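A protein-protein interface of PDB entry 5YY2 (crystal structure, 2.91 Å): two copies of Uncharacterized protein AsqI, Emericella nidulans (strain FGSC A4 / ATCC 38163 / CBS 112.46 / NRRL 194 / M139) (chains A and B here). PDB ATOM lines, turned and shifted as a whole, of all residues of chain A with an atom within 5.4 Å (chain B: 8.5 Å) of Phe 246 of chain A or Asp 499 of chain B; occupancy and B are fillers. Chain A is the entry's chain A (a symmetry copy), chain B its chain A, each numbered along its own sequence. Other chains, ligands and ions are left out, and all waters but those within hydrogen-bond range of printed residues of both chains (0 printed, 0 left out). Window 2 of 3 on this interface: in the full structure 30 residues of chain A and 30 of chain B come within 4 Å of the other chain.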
ATOM      1  N   ARG A 238       6.950 -26.187  21.458  1.00  0.00           N
ATOM      2  CA  ARG A 238       7.851 -26.717  22.459  1.00  0.00           C
ATOM      3  C   ARG A 238       7.735 -25.873  23.698  1.00  0.00           C
ATOM      4  O   ARG A 238       8.008 -24.688  23.656  1.00  0.00           O
ATOM      5  CB  ARG A 238       9.287 -26.712  21.959  1.00  0.00           C
ATOM      6  CG  ARG A 238      10.292 -27.250  22.962  1.00  0.00           C
ATOM      7  CD  ARG A 238      11.699 -26.645  22.772  1.00  0.00           C
ATOM      8  NE  ARG A 238      11.963 -26.271  21.393  1.00  0.00           N
ATOM      9  CZ  ARG A 238      12.730 -25.249  21.047  1.00  0.00           C
ATOM     10  NH1 ARG A 238      13.305 -24.513  21.982  1.00  0.00           N
ATOM     11  NH2 ARG A 238      12.922 -24.958  19.775  1.00  0.00           N
ATOM     12  N   TRP A 240       8.254 -23.958  27.226  1.00  0.00           N
ATOM     13  CA  TRP A 240       9.363 -23.282  27.860  1.00  0.00           C
ATOM     14  C   TRP A 240       9.668 -23.961  29.174  1.00  0.00           C
ATOM     15  O   TRP A 240       9.535 -23.373  30.224  1.00  0.00           O
ATOM     16  CB  TRP A 240       9.010 -21.825  28.089  1.00  0.00           C
ATOM     17  CG  TRP A 240      10.132 -20.945  28.459  1.00  0.00           C
ATOM     18  CD1 TRP A 240      10.403 -20.441  29.689  1.00  0.00           C
ATOM     19  CD2 TRP A 240      11.130 -20.432  27.586  1.00  0.00           C
ATOM     20  NE1 TRP A 240      11.517 -19.652  29.642  1.00  0.00           N
ATOM     21  CE2 TRP A 240      11.984 -19.629  28.357  1.00  0.00           C
ATOM     22  CE3 TRP A 240      11.386 -20.567  26.221  1.00  0.00           C
ATOM     23  CZ2 TRP A 240      13.068 -18.968  27.813  1.00  0.00           C
ATOM     24  CZ3 TRP A 240      12.470 -19.909  25.688  1.00  0.00           C
ATOM     25  CH2 TRP A 240      13.298 -19.126  26.483  1.00  0.00           C
ATOM     26  N   ASP A 244      16.885 -22.286  29.841  1.00  0.00           N
ATOM     27  CA  ASP A 244      18.085 -21.886  29.150  1.00  0.00           C
ATOM     28  C   ASP A 244      17.892 -22.131  27.658  1.00  0.00           C
ATOM     29  O   ASP A 244      18.838 -22.295  26.892  1.00  0.00           O
ATOM     30  CB  ASP A 244      19.282 -22.648  29.703  1.00  0.00           C
ATOM     31  CG  ASP A 244      19.083 -24.138  29.684  1.00  0.00           C
ATOM     32  OD1 ASP A 244      18.045 -24.600  29.185  1.00  0.00           O
ATOM     33  OD2 ASP A 244      19.976 -24.856  30.158  1.00  0.00           O
ATOM     34  N   ASP A 245      16.633 -22.162  27.267  1.00  0.00           N
ATOM     35  CA  ASP A 245      16.253 -22.515  25.928  1.00  0.00           C
ATOM     36  C   ASP A 245      16.384 -21.289  25.052  1.00  0.00           C
ATOM     37  O   ASP A 245      16.406 -20.169  25.536  1.00  0.00           O
ATOM     38  CB  ASP A 245      14.825 -23.060  25.913  1.00  0.00           C
ATOM     39  CG  ASP A 245      14.589 -24.069  24.817  1.00  0.00           C
ATOM     40  OD1 ASP A 245      15.424 -24.152  23.900  1.00  0.00           O
ATOM     41  OD2 ASP A 245      13.559 -24.772  24.872  1.00  0.00           O
ATOM     42  N   PHE A 246      16.487 -21.513  23.752  1.00  0.00           N
ATOM     43  CA  PHE A 246      16.563 -20.442  22.787  1.00  0.00           C
ATOM     44  C   PHE A 246      15.188 -20.127  22.225  1.00  0.00           C
ATOM     45  O   PHE A 246      14.331 -20.993  22.136  1.00  0.00           O
ATOM     46  CB  PHE A 246      17.484 -20.822  21.644  1.00  0.00           C
ATOM     47  CG  PHE A 246      18.892 -21.067  22.051  1.00  0.00           C
ATOM     48  CD1 PHE A 246      19.750 -20.014  22.266  1.00  0.00           C
ATOM     49  CD2 PHE A 246      19.369 -22.346  22.184  1.00  0.00           C
ATOM     50  CE1 PHE A 246      21.044 -20.229  22.630  1.00  0.00           C
ATOM     51  CE2 PHE A 246      20.657 -22.568  22.544  1.00  0.00           C
ATOM     52  CZ  PHE A 246      21.501 -21.507  22.768  1.00  0.00           C
ATOM     53  N   LEU A 247      14.979 -18.874  21.859  1.00  0.00           N
ATOM     54  CA  LEU A 247      13.853 -18.525  21.032  1.00  0.00           C
ATOM     55  C   LEU A 247      14.373 -18.442  19.607  1.00  0.00           C
ATOM     56  O   LEU A 247      14.766 -17.391  19.138  1.00  0.00           O
ATOM     57  CB  LEU A 247      13.218 -17.220  21.485  1.00  0.00           C
ATOM     58  CG  LEU A 247      12.415 -17.306  22.779  1.00  0.00           C
ATOM     59  CD1 LEU A 247      12.250 -15.959  23.391  1.00  0.00           C
ATOM     60  CD2 LEU A 247      11.070 -17.899  22.517  1.00  0.00           C
ATOM     61  N   GLU A 248      14.368 -19.574  18.921  1.00  0.00           N
ATOM     62  CA  GLU A 248      15.111 -19.725  17.684  1.00  0.00           C
ATOM     63  C   GLU A 248      14.514 -19.024  16.483  1.00  0.00           C
ATOM     64  O   GLU A 248      15.084 -19.063  15.416  1.00  0.00           O
ATOM     65  CB  GLU A 248      15.250 -21.197  17.353  1.00  0.00           C
ATOM     66  CG  GLU A 248      13.988 -21.786  16.804  1.00  0.00           C
ATOM     67  CD  GLU A 248      13.435 -22.892  17.668  1.00  0.00           C
ATOM     68  OE1 GLU A 248      12.798 -22.580  18.700  1.00  0.00           O
ATOM     69  OE2 GLU A 248      13.634 -24.071  17.308  1.00  0.00           O
ATOM     70  N   PHE A 267      17.220 -16.768  18.300  1.00  0.00           N
ATOM     71  CA  PHE A 267      18.024 -17.417  19.331  1.00  0.00           C
ATOM     72  C   PHE A 267      18.312 -16.533  20.544  1.00  0.00           C
ATOM     73  O   PHE A 267      19.310 -16.721  21.212  1.00  0.00           O
ATOM     74  CB  PHE A 267      19.326 -17.920  18.737  1.00  0.00           C
ATOM     75  CG  PHE A 267      19.149 -19.008  17.748  1.00  0.00           C
ATOM     76  CD1 PHE A 267      18.971 -18.725  16.421  1.00  0.00           C
ATOM     77  CD2 PHE A 267      19.170 -20.320  18.147  1.00  0.00           C
ATOM     78  CE1 PHE A 267      18.808 -19.733  15.510  1.00  0.00           C
ATOM     79  CE2 PHE A 267      19.013 -21.330  17.237  1.00  0.00           C
ATOM     80  CZ  PHE A 267      18.829 -21.035  15.921  1.00  0.00           C
ATOM     81  N   SER A 268      17.427 -15.586  20.826  1.00  0.00           N
ATOM     82  CA  SER A 268      17.498 -14.823  22.055  1.00  0.00           C
ATOM     83  C   SER A 268      17.236 -15.747  23.217  1.00  0.00           C
ATOM     84  O   SER A 268      16.550 -16.734  23.065  1.00  0.00           O
ATOM     85  CB  SER A 268      16.489 -13.692  22.047  1.00  0.00           C
ATOM     86  OG  SER A 268      16.392 -13.135  20.761  1.00  0.00           O
ATOM     87  N   THR A 269      17.785 -15.439  24.381  1.00  0.00           N
ATOM     88  CA  THR A 269      17.513 -16.238  25.560  1.00  0.00           C
ATOM     89  C   THR A 269      17.103 -15.320  26.693  1.00  0.00           C
ATOM     90  O   THR A 269      17.010 -14.129  26.506  1.00  0.00           O
ATOM     91  CB  THR A 269      18.729 -17.077  25.972  1.00  0.00           C
ATOM     92  OG1 THR A 269      19.786 -16.225  26.403  1.00  0.00           O
ATOM     93  CG2 THR A 269      19.233 -17.880  24.820  1.00  0.00           C
ATOM     94  N   ARG A 395       4.802 -19.954  24.419  1.00  0.00           N
ATOM     95  CA  ARG A 395       5.698 -21.005  24.826  1.00  0.00           C
ATOM     96  C   ARG A 395       5.754 -21.004  26.314  1.00  0.00           C
ATOM     97  O   ARG A 395       6.046 -22.008  26.929  1.00  0.00           O
ATOM     98  CB  ARG A 395       7.065 -20.810  24.248  1.00  0.00           C
ATOM     99  CG  ARG A 395       7.112 -21.033  22.796  1.00  0.00           C
ATOM    100  CD  ARG A 395       8.532 -21.198  22.392  1.00  0.00           C
ATOM    101  NE  ARG A 395       9.114 -22.317  23.094  1.00  0.00           N
ATOM    102  CZ  ARG A 395      10.410 -22.522  23.180  1.00  0.00           C
ATOM    103  NH1 ARG A 395      11.235 -21.666  22.613  1.00  0.00           N
ATOM    104  NH2 ARG A 395      10.879 -23.569  23.823  1.00  0.00           N
ATOM    105  N   GLU B 226      21.296 -32.112  17.250  1.00  0.00           N
ATOM    106  CA  GLU B 226      20.628 -30.836  17.232  1.00  0.00           C
ATOM    107  C   GLU B 226      21.315 -29.873  16.298  1.00  0.00           C
ATOM    108  O   GLU B 226      20.667 -29.096  15.620  1.00  0.00           O
ATOM    109  CB  GLU B 226      20.573 -30.249  18.622  1.00  0.00           C
ATOM    110  CG  GLU B 226      19.446 -30.782  19.426  1.00  0.00           C
ATOM    111  CD  GLU B 226      18.875 -29.740  20.339  1.00  0.00           C
ATOM    112  OE1 GLU B 226      19.625 -29.256  21.208  1.00  0.00           O
ATOM    113  OE2 GLU B 226      17.685 -29.400  20.174  1.00  0.00           O
ATOM    114  N   THR B 227      22.638 -29.923  16.257  1.00  0.00           N
ATOM    115  CA  THR B 227      23.389 -29.035  15.379  1.00  0.00           C
ATOM    116  C   THR B 227      23.117 -29.420  13.934  1.00  0.00           C
ATOM    117  O   THR B 227      22.784 -28.570  13.122  1.00  0.00           O
ATOM    118  CB  THR B 227      24.901 -29.072  15.683  1.00  0.00           C
ATOM    119  OG1 THR B 227      25.117 -28.604  17.018  1.00  0.00           O
ATOM    120  CG2 THR B 227      25.661 -28.165  14.751  1.00  0.00           C
ATOM    121  N   LEU B 230      19.865 -28.051  12.899  1.00  0.00           N
ATOM    122  CA  LEU B 230      19.968 -26.633  12.563  1.00  0.00           C
ATOM    123  C   LEU B 230      20.605 -26.383  11.203  1.00  0.00           C
ATOM    124  O   LEU B 230      20.387 -25.352  10.582  1.00  0.00           O
ATOM    125  CB  LEU B 230      20.788 -25.923  13.629  1.00  0.00           C
ATOM    126  CG  LEU B 230      20.381 -24.542  14.123  1.00  0.00           C
ATOM    127  CD1 LEU B 230      21.157 -24.249  15.379  1.00  0.00           C
ATOM    128  CD2 LEU B 230      20.642 -23.475  13.093  1.00  0.00           C
ATOM    129  N   CYS B 231      21.417 -27.324  10.749  1.00  0.00           N
ATOM    130  CA  CYS B 231      22.158 -27.135   9.517  1.00  0.00           C
ATOM    131  C   CYS B 231      21.235 -27.154   8.306  1.00  0.00           C
ATOM    132  O   CYS B 231      21.473 -26.466   7.331  1.00  0.00           O
ATOM    133  CB  CYS B 231      23.236 -28.204   9.376  1.00  0.00           C
ATOM    134  SG  CYS B 231      24.611 -28.078  10.521  1.00  0.00           S
ATOM    135  N   SER B 233      18.208 -26.290   8.696  1.00  0.00           N
ATOM    136  CA  SER B 233      17.175 -25.392   9.195  1.00  0.00           C
ATOM    137  C   SER B 233      15.912 -26.141   9.615  1.00  0.00           C
ATOM    138  O   SER B 233      14.812 -25.662   9.428  1.00  0.00           O
ATOM    139  CB  SER B 233      16.846 -24.344   8.141  1.00  0.00           C
ATOM    140  OG  SER B 233      18.018 -23.715   7.659  1.00  0.00           O
ATOM    141  N   LEU B 236      14.390 -27.205  16.209  1.00  0.00           N
ATOM    142  CA  LEU B 236      15.172 -27.788  17.278  1.00  0.00           C
ATOM    143  C   LEU B 236      14.389 -28.939  17.887  1.00  0.00           C
ATOM    144  O   LEU B 236      13.167 -28.916  17.905  1.00  0.00           O
ATOM    145  CB  LEU B 236      15.505 -26.733  18.326  1.00  0.00           C
ATOM    146  CG  LEU B 236      16.643 -25.768  18.007  1.00  0.00           C
ATOM    147  CD1 LEU B 236      16.713 -24.680  19.047  1.00  0.00           C
ATOM    148  CD2 LEU B 236      17.978 -26.489  17.936  1.00  0.00           C
ATOM    149  N   ARG B 405      21.602 -30.670  32.338  1.00  0.00           N
ATOM    150  CA  ARG B 405      21.447 -29.228  32.409  1.00  0.00           C
ATOM    151  C   ARG B 405      21.092 -28.755  33.793  1.00  0.00           C
ATOM    152  O   ARG B 405      21.455 -27.659  34.192  1.00  0.00           O
ATOM    153  CB  ARG B 405      20.370 -28.753  31.452  1.00  0.00           C
ATOM    154  CG  ARG B 405      20.728 -28.876  30.032  1.00  0.00           C
ATOM    155  CD  ARG B 405      19.586 -28.430  29.177  1.00  0.00           C
ATOM    156  NE  ARG B 405      19.944 -28.585  27.785  1.00  0.00           N
ATOM    157  CZ  ARG B 405      20.471 -27.617  27.058  1.00  0.00           C
ATOM    158  NH1 ARG B 405      20.662 -26.420  27.591  1.00  0.00           N
ATOM    159  NH2 ARG B 405      20.789 -27.849  25.802  1.00  0.00           N
ATOM    160  N   ALA B 496      31.126 -25.123  18.272  1.00  0.00           N
ATOM    161  CA  ALA B 496      29.712 -24.847  18.463  1.00  0.00           C
ATOM    162  C   ALA B 496      29.154 -24.046  17.298  1.00  0.00           C
ATOM    163  O   ALA B 496      29.855 -23.244  16.711  1.00  0.00           O
ATOM    164  CB  ALA B 496      29.488 -24.110  19.739  1.00  0.00           C
ATOM    165  N   ALA B 497      27.891 -24.275  16.968  1.00  0.00           N
ATOM    166  CA  ALA B 497      27.218 -23.441  16.003  1.00  0.00           C
ATOM    167  C   ALA B 497      27.065 -22.080  16.622  1.00  0.00           C
ATOM    168  O   ALA B 497      26.572 -21.960  17.727  1.00  0.00           O
ATOM    169  CB  ALA B 497      25.880 -24.012  15.618  1.00  0.00           C
ATOM    170  N   GLU B 498      27.486 -21.055  15.899  1.00  0.00           N
ATOM    171  CA  GLU B 498      27.478 -19.692  16.400  1.00  0.00           C
ATOM    172  C   GLU B 498      26.167 -19.348  17.081  1.00  0.00           C
ATOM    173  O   GLU B 498      26.127 -18.569  18.021  1.00  0.00           O
ATOM    174  CB  GLU B 498      27.755 -18.723  15.264  1.00  0.00           C
ATOM    175  CG  GLU B 498      28.172 -17.356  15.730  1.00  0.00           C
ATOM    176  CD  GLU B 498      28.575 -16.438  14.600  1.00  0.00           C
ATOM    177  OE1 GLU B 498      29.289 -16.881  13.680  1.00  0.00           O
ATOM    178  OE2 GLU B 498      28.170 -15.264  14.639  1.00  0.00           O
ATOM    179  N   ASP B 499      25.094 -19.969  16.623  1.00  0.00           N
ATOM    180  CA  ASP B 499      23.774 -19.697  17.154  1.00  0.00           C
ATOM    181  C   ASP B 499      23.624 -20.290  18.532  1.00  0.00           C
ATOM    182  O   ASP B 499      23.012 -19.694  19.403  1.00  0.00           O
ATOM    183  CB  ASP B 499      22.706 -20.245  16.223  1.00  0.00           C
ATOM    184  CG  ASP B 499      22.455 -19.352  15.032  1.00  0.00           C
ATOM    185  OD1 ASP B 499      22.604 -18.126  15.159  1.00  0.00           O
ATOM    186  OD2 ASP B 499      22.104 -19.878  13.960  1.00  0.00           O
ATOM    187  N   LEU B 500      24.215 -21.456  18.736  1.00  0.00           N
ATOM    188  CA  LEU B 500      24.004 -22.208  19.964  1.00  0.00           C
ATOM    189  C   LEU B 500      25.167 -22.055  20.902  1.00  0.00           C
ATOM    190  O   LEU B 500      25.428 -22.913  21.719  1.00  0.00           O
ATOM    191  CB  LEU B 500      23.799 -23.684  19.654  1.00  0.00           C
ATOM    192  CG  LEU B 500      22.769 -24.063  18.608  1.00  0.00           C
ATOM    193  CD1 LEU B 500      22.915 -25.511  18.272  1.00  0.00           C
ATOM    194  CD2 LEU B 500      21.390 -23.764  19.122  1.00  0.00           C
ATOM    195  N   MET B 501      25.853 -20.937  20.777  1.00  0.00           N
ATOM    196  CA  MET B 501      27.175 -20.768  21.349  1.00  0.00           C
ATOM    197  C   MET B 501      27.129 -20.524  22.841  1.00  0.00           C
ATOM    198  O   MET B 501      28.006 -20.946  23.582  1.00  0.00           O
ATOM    199  CB  MET B 501      27.877 -19.613  20.640  1.00  0.00           C
ATOM    200  CG  MET B 501      29.252 -19.272  21.149  1.00  0.00           C
ATOM    201  SD  MET B 501      29.935 -17.888  20.259  1.00  0.00           S
ATOM    202  CE  MET B 501      28.497 -16.880  20.049  1.00  0.00           C
ATOM    203  N   ASN B 502      26.088 -19.841  23.282  1.00  0.00           N
ATOM    204  CA  ASN B 502      26.004 -19.425  24.666  1.00  0.00           C
ATOM    205  C   ASN B 502      25.318 -20.453  25.544  1.00  0.00           C
ATOM    206  O   ASN B 502      24.936 -20.177  26.674  1.00  0.00           O
ATOM    207  CB  ASN B 502      25.304 -18.079  24.749  1.00  0.00           C
ATOM    208  CG  ASN B 502      26.174 -16.963  24.220  1.00  0.00           C
ATOM    209  OD1 ASN B 502      27.390 -17.072  24.243  1.00  0.00           O
ATOM    210  ND2 ASN B 502      25.565 -15.895  23.733  1.00  0.00           N
ATOM    211  N   ASP B 503      25.209 -21.657  25.014  1.00  0.00           N
ATOM    212  CA  ASP B 503      24.718 -22.783  25.765  1.00  0.00           C
ATOM    213  C   ASP B 503      25.843 -23.767  26.010  1.00  0.00           C
ATOM    214  O   ASP B 503      26.413 -24.270  25.072  1.00  0.00           O
ATOM    215  CB  ASP B 503      23.593 -23.464  25.016  1.00  0.00           C
ATOM    216  CG  ASP B 503      23.150 -24.724  25.680  1.00  0.00           C
ATOM    217  OD1 ASP B 503      23.248 -24.791  26.915  1.00  0.00           O
ATOM    218  OD2 ASP B 503      22.716 -25.642  24.963  1.00  0.00           O
ATOM    219  N   TYR B 504      26.148 -24.056  27.269  1.00  0.00           N
ATOM    220  CA  TYR B 504      27.252 -24.937  27.601  1.00  0.00           C
ATOM    221  C   TYR B 504      27.161 -26.255  26.897  1.00  0.00           C
ATOM    222  O   TYR B 504      28.168 -26.847  26.539  1.00  0.00           O
ATOM    223  CB  TYR B 504      27.306 -25.237  29.081  1.00  0.00           C
ATOM    224  CG  TYR B 504      27.448 -24.055  29.981  1.00  0.00           C
ATOM    225  CD1 TYR B 504      28.691 -23.570  30.318  1.00  0.00           C
ATOM    226  CD2 TYR B 504      26.341 -23.444  30.522  1.00  0.00           C
ATOM    227  CE1 TYR B 504      28.818 -22.505  31.155  1.00  0.00           C
ATOM    228  CE2 TYR B 504      26.464 -22.390  31.357  1.00  0.00           C
ATOM    229  CZ  TYR B 504      27.700 -21.923  31.670  1.00  0.00           C
ATOM    230  OH  TYR B 504      27.826 -20.859  32.508  1.00  0.00           O
ATOM    231  N   HIS B 505      25.942 -26.725  26.698  1.00  0.00           N
ATOM    232  CA  HIS B 505      25.754 -28.123  26.362  1.00  0.00           C
ATOM    233  C   HIS B 505      25.692 -28.395  24.881  1.00  0.00           C
ATOM    234  O   HIS B 505      25.467 -29.522  24.488  1.00  0.00           O
ATOM    235  CB  HIS B 505      24.490 -28.642  27.025  1.00  0.00           C
ATOM    236  CG  HIS B 505      24.492 -28.491  28.507  1.00  0.00           C
ATOM    237  ND1 HIS B 505      25.122 -29.383  29.344  1.00  0.00           N
ATOM    238  CD2 HIS B 505      23.953 -27.542  29.300  1.00  0.00           C
ATOM    239  CE1 HIS B 505      24.969 -28.990  30.592  1.00  0.00           C
ATOM    240  NE2 HIS B 505      24.262 -27.875  30.593  1.00  0.00           N
ATOM    241  N   SER B 506      25.912 -27.375  24.062  1.00  0.00           N
ATOM    242  CA  SER B 506      25.867 -27.544  22.624  1.00  0.00           C
ATOM    243  C   SER B 506      27.257 -27.618  22.063  1.00  0.00           C
ATOM    244  O   SER B 506      27.454 -27.992  20.930  1.00  0.00           O
ATOM    245  CB  SER B 506      25.097 -26.416  21.975  1.00  0.00           C
ATOM    246  OG  SER B 506      23.761 -26.390  22.455  1.00  0.00           O
ATOM    247  N   LYS B 567      26.042 -25.704   5.755  1.00  0.00           N
ATOM    248  CA  LYS B 567      25.089 -25.166   4.818  1.00  0.00           C
ATOM    249  C   LYS B 567      25.808 -24.844   3.535  1.00  0.00           C
ATOM    250  O   LYS B 567      27.015 -24.741   3.526  1.00  0.00           O
ATOM    251  CB  LYS B 567      24.419 -23.931   5.388  1.00  0.00           C
ATOM    252  CG  LYS B 567      23.528 -24.235   6.548  1.00  0.00           C
ATOM    253  CD  LYS B 567      22.984 -23.003   7.178  1.00  0.00           C
ATOM    254  CE  LYS B 567      21.842 -23.327   8.093  1.00  0.00           C
ATOM    255  NZ  LYS B 567      21.319 -22.099   8.723  1.00  0.00           N
ATOM    256  N   MET B 571      28.223 -22.336   6.737  1.00  0.00           N
ATOM    257  CA  MET B 571      27.572 -22.082   8.005  1.00  0.00           C
ATOM    258  C   MET B 571      28.605 -21.671   9.023  1.00  0.00           C
ATOM    259  O   MET B 571      29.639 -22.293   9.114  1.00  0.00           O
ATOM    260  CB  MET B 571      26.816 -23.327   8.466  1.00  0.00           C
ATOM    261  CG  MET B 571      25.976 -23.140   9.709  1.00  0.00           C
ATOM    262  SD  MET B 571      25.274 -24.672  10.310  1.00  0.00           S
ATOM    263  CE  MET B 571      24.271 -24.068  11.630  1.00  0.00           C
ATOM    264  N   PRO B 572      28.338 -20.608   9.781  1.00  0.00           N
ATOM    265  CA  PRO B 572      29.305 -20.166  10.777  1.00  0.00           C
ATOM    266  C   PRO B 572      29.344 -21.067  11.998  1.00  0.00           C
ATOM    267  O   PRO B 572      28.313 -21.442  12.514  1.00  0.00           O
ATOM    268  CB  PRO B 572      28.807 -18.773  11.141  1.00  0.00           C
ATOM    269  CG  PRO B 572      27.382 -18.814  10.893  1.00  0.00           C
ATOM    270  CD  PRO B 572      27.200 -19.688   9.694  1.00  0.00           C
ATOM    271  N   PHE B 573      30.550 -21.413  12.428  1.00  0.00           N
ATOM    272  CA  PHE B 573      30.799 -22.172  13.637  1.00  0.00           C
ATOM    273  C   PHE B 573      31.867 -21.458  14.442  1.00  0.00           C
ATOM    274  O   PHE B 573      32.586 -20.627  13.924  1.00  0.00           O
ATOM    275  CB  PHE B 573      31.258 -23.587  13.322  1.00  0.00           C
ATOM    276  CG  PHE B 573      30.141 -24.550  13.081  1.00  0.00           C
ATOM    277  CD1 PHE B 573      29.605 -24.706  11.823  1.00  0.00           C
ATOM    278  CD2 PHE B 573      29.632 -25.301  14.105  1.00  0.00           C
ATOM    279  CE1 PHE B 573      28.588 -25.572  11.594  1.00  0.00           C
ATOM    280  CE2 PHE B 573      28.607 -26.168  13.876  1.00  0.00           C
ATOM    281  CZ  PHE B 573      28.091 -26.301  12.612  1.00  0.00           C
ATOM    282  N   VAL B 574      31.964 -21.779  15.720  1.00  0.00           N
ATOM    283  CA  VAL B 574      33.015 -21.228  16.540  1.00  0.00           C
ATOM    284  C   VAL B 574      33.859 -22.368  17.075  1.00  0.00           C
ATOM    285  O   VAL B 574      33.333 -23.397  17.450  1.00  0.00           O
ATOM    286  CB  VAL B 574      32.444 -20.391  17.669  1.00  0.00           C
ATOM    287  CG1 VAL B 574      33.538 -19.801  18.498  1.00  0.00           C
ATOM    288  CG2 VAL B 574      31.603 -19.287  17.095  1.00  0.00           C
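The backbone NH (N) of Leu 236 of chain B lies within hydrogen-bond range of the side-chain carboxylate (OE2) of Glu 248 of chain A (3.4 Å). NH1 of Arg 405 of chain B is in salt-bridge range of OD2 of Asp 244 of chain A, 3.1 Å away.
The backbone carbonyl oxygen (O) of Phe 246 of chain A sits at hydrogen-bond distance from the guanidinium group (NH1) of Arg 395 of chain A, at 3.2 Å. O of Arg 238 of chain A lies within hydrogen-bond range of NE of Arg 395 of chain A (2.7 Å). The guanidinium group (NH1) of Arg 238 of chain A lies within salt-bridge range of the side-chain carboxylate (OD1) of Asp 245 of chain A (2.9 Å). OD2 of Asp 503 of chain B is in hydrogen-bond range of OG of Ser 506 of chain B. NH2 of Arg 238 of chain A lies within salt-bridge range of OE1 of Glu 248 of chain A. NH2 of Arg 405 of chain B lies within salt-bridge range of OD2 of Asp 503 of chain B, at 3.0 Å.
Among the printed residues, merely in contact across the chains: Arg 238 of chain A with Leu 236 of chain B (3.5 Å), Phe 246 of chain A with Asp 503 of chain B (3.6 Å), Phe 267 of chain A with Asp 499 of chain B (3.6 Å), Phe 246 of chain A with Leu 500 of chain B (3.7 Å), Phe 246 of chain A with Asp 499 of chain B (3.8 Å) and Phe 267 of chain A with Leu 500 of chain B (3.9 Å).
Phe 246 of chain A touches just these residues of chain B: Asp 499, Leu 500 and Asp 503. Of the printed residues of chain A, Arg 405 of chain B touches Asp 244 (3.1 Å). Printed residues of chain B within 4 Å of Glu 248 of chain A: Leu 236 (3.4 Å). Trp 240 of chain A touches none of the printed residues of chain B. Leu 247 of chain A touches none of the printed residues of chain B. The nearest printed residue of chain A that does not touch Arg 405 of chain B is Asp 245 of chain A (5.9 Å).
Of the 11 printed residues of chain A, 5 touch a printed residue of chain B. Hydrophobic or aromatic side chains of chain A within 4 Å of the printed part of chain B: Phe 246 and Phe 267. Printed residues of chain B that touch a printed residue of chain A: Leu 236, Arg 405, Asp 499, Leu 500 and Asp 503. Among the printed residues, 8 pairs touch across the chains.
No position is printed for both chains. Of the 8 pairs that touch across the chains among the printed residues, none has its exchanged pair printed and touching as well.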
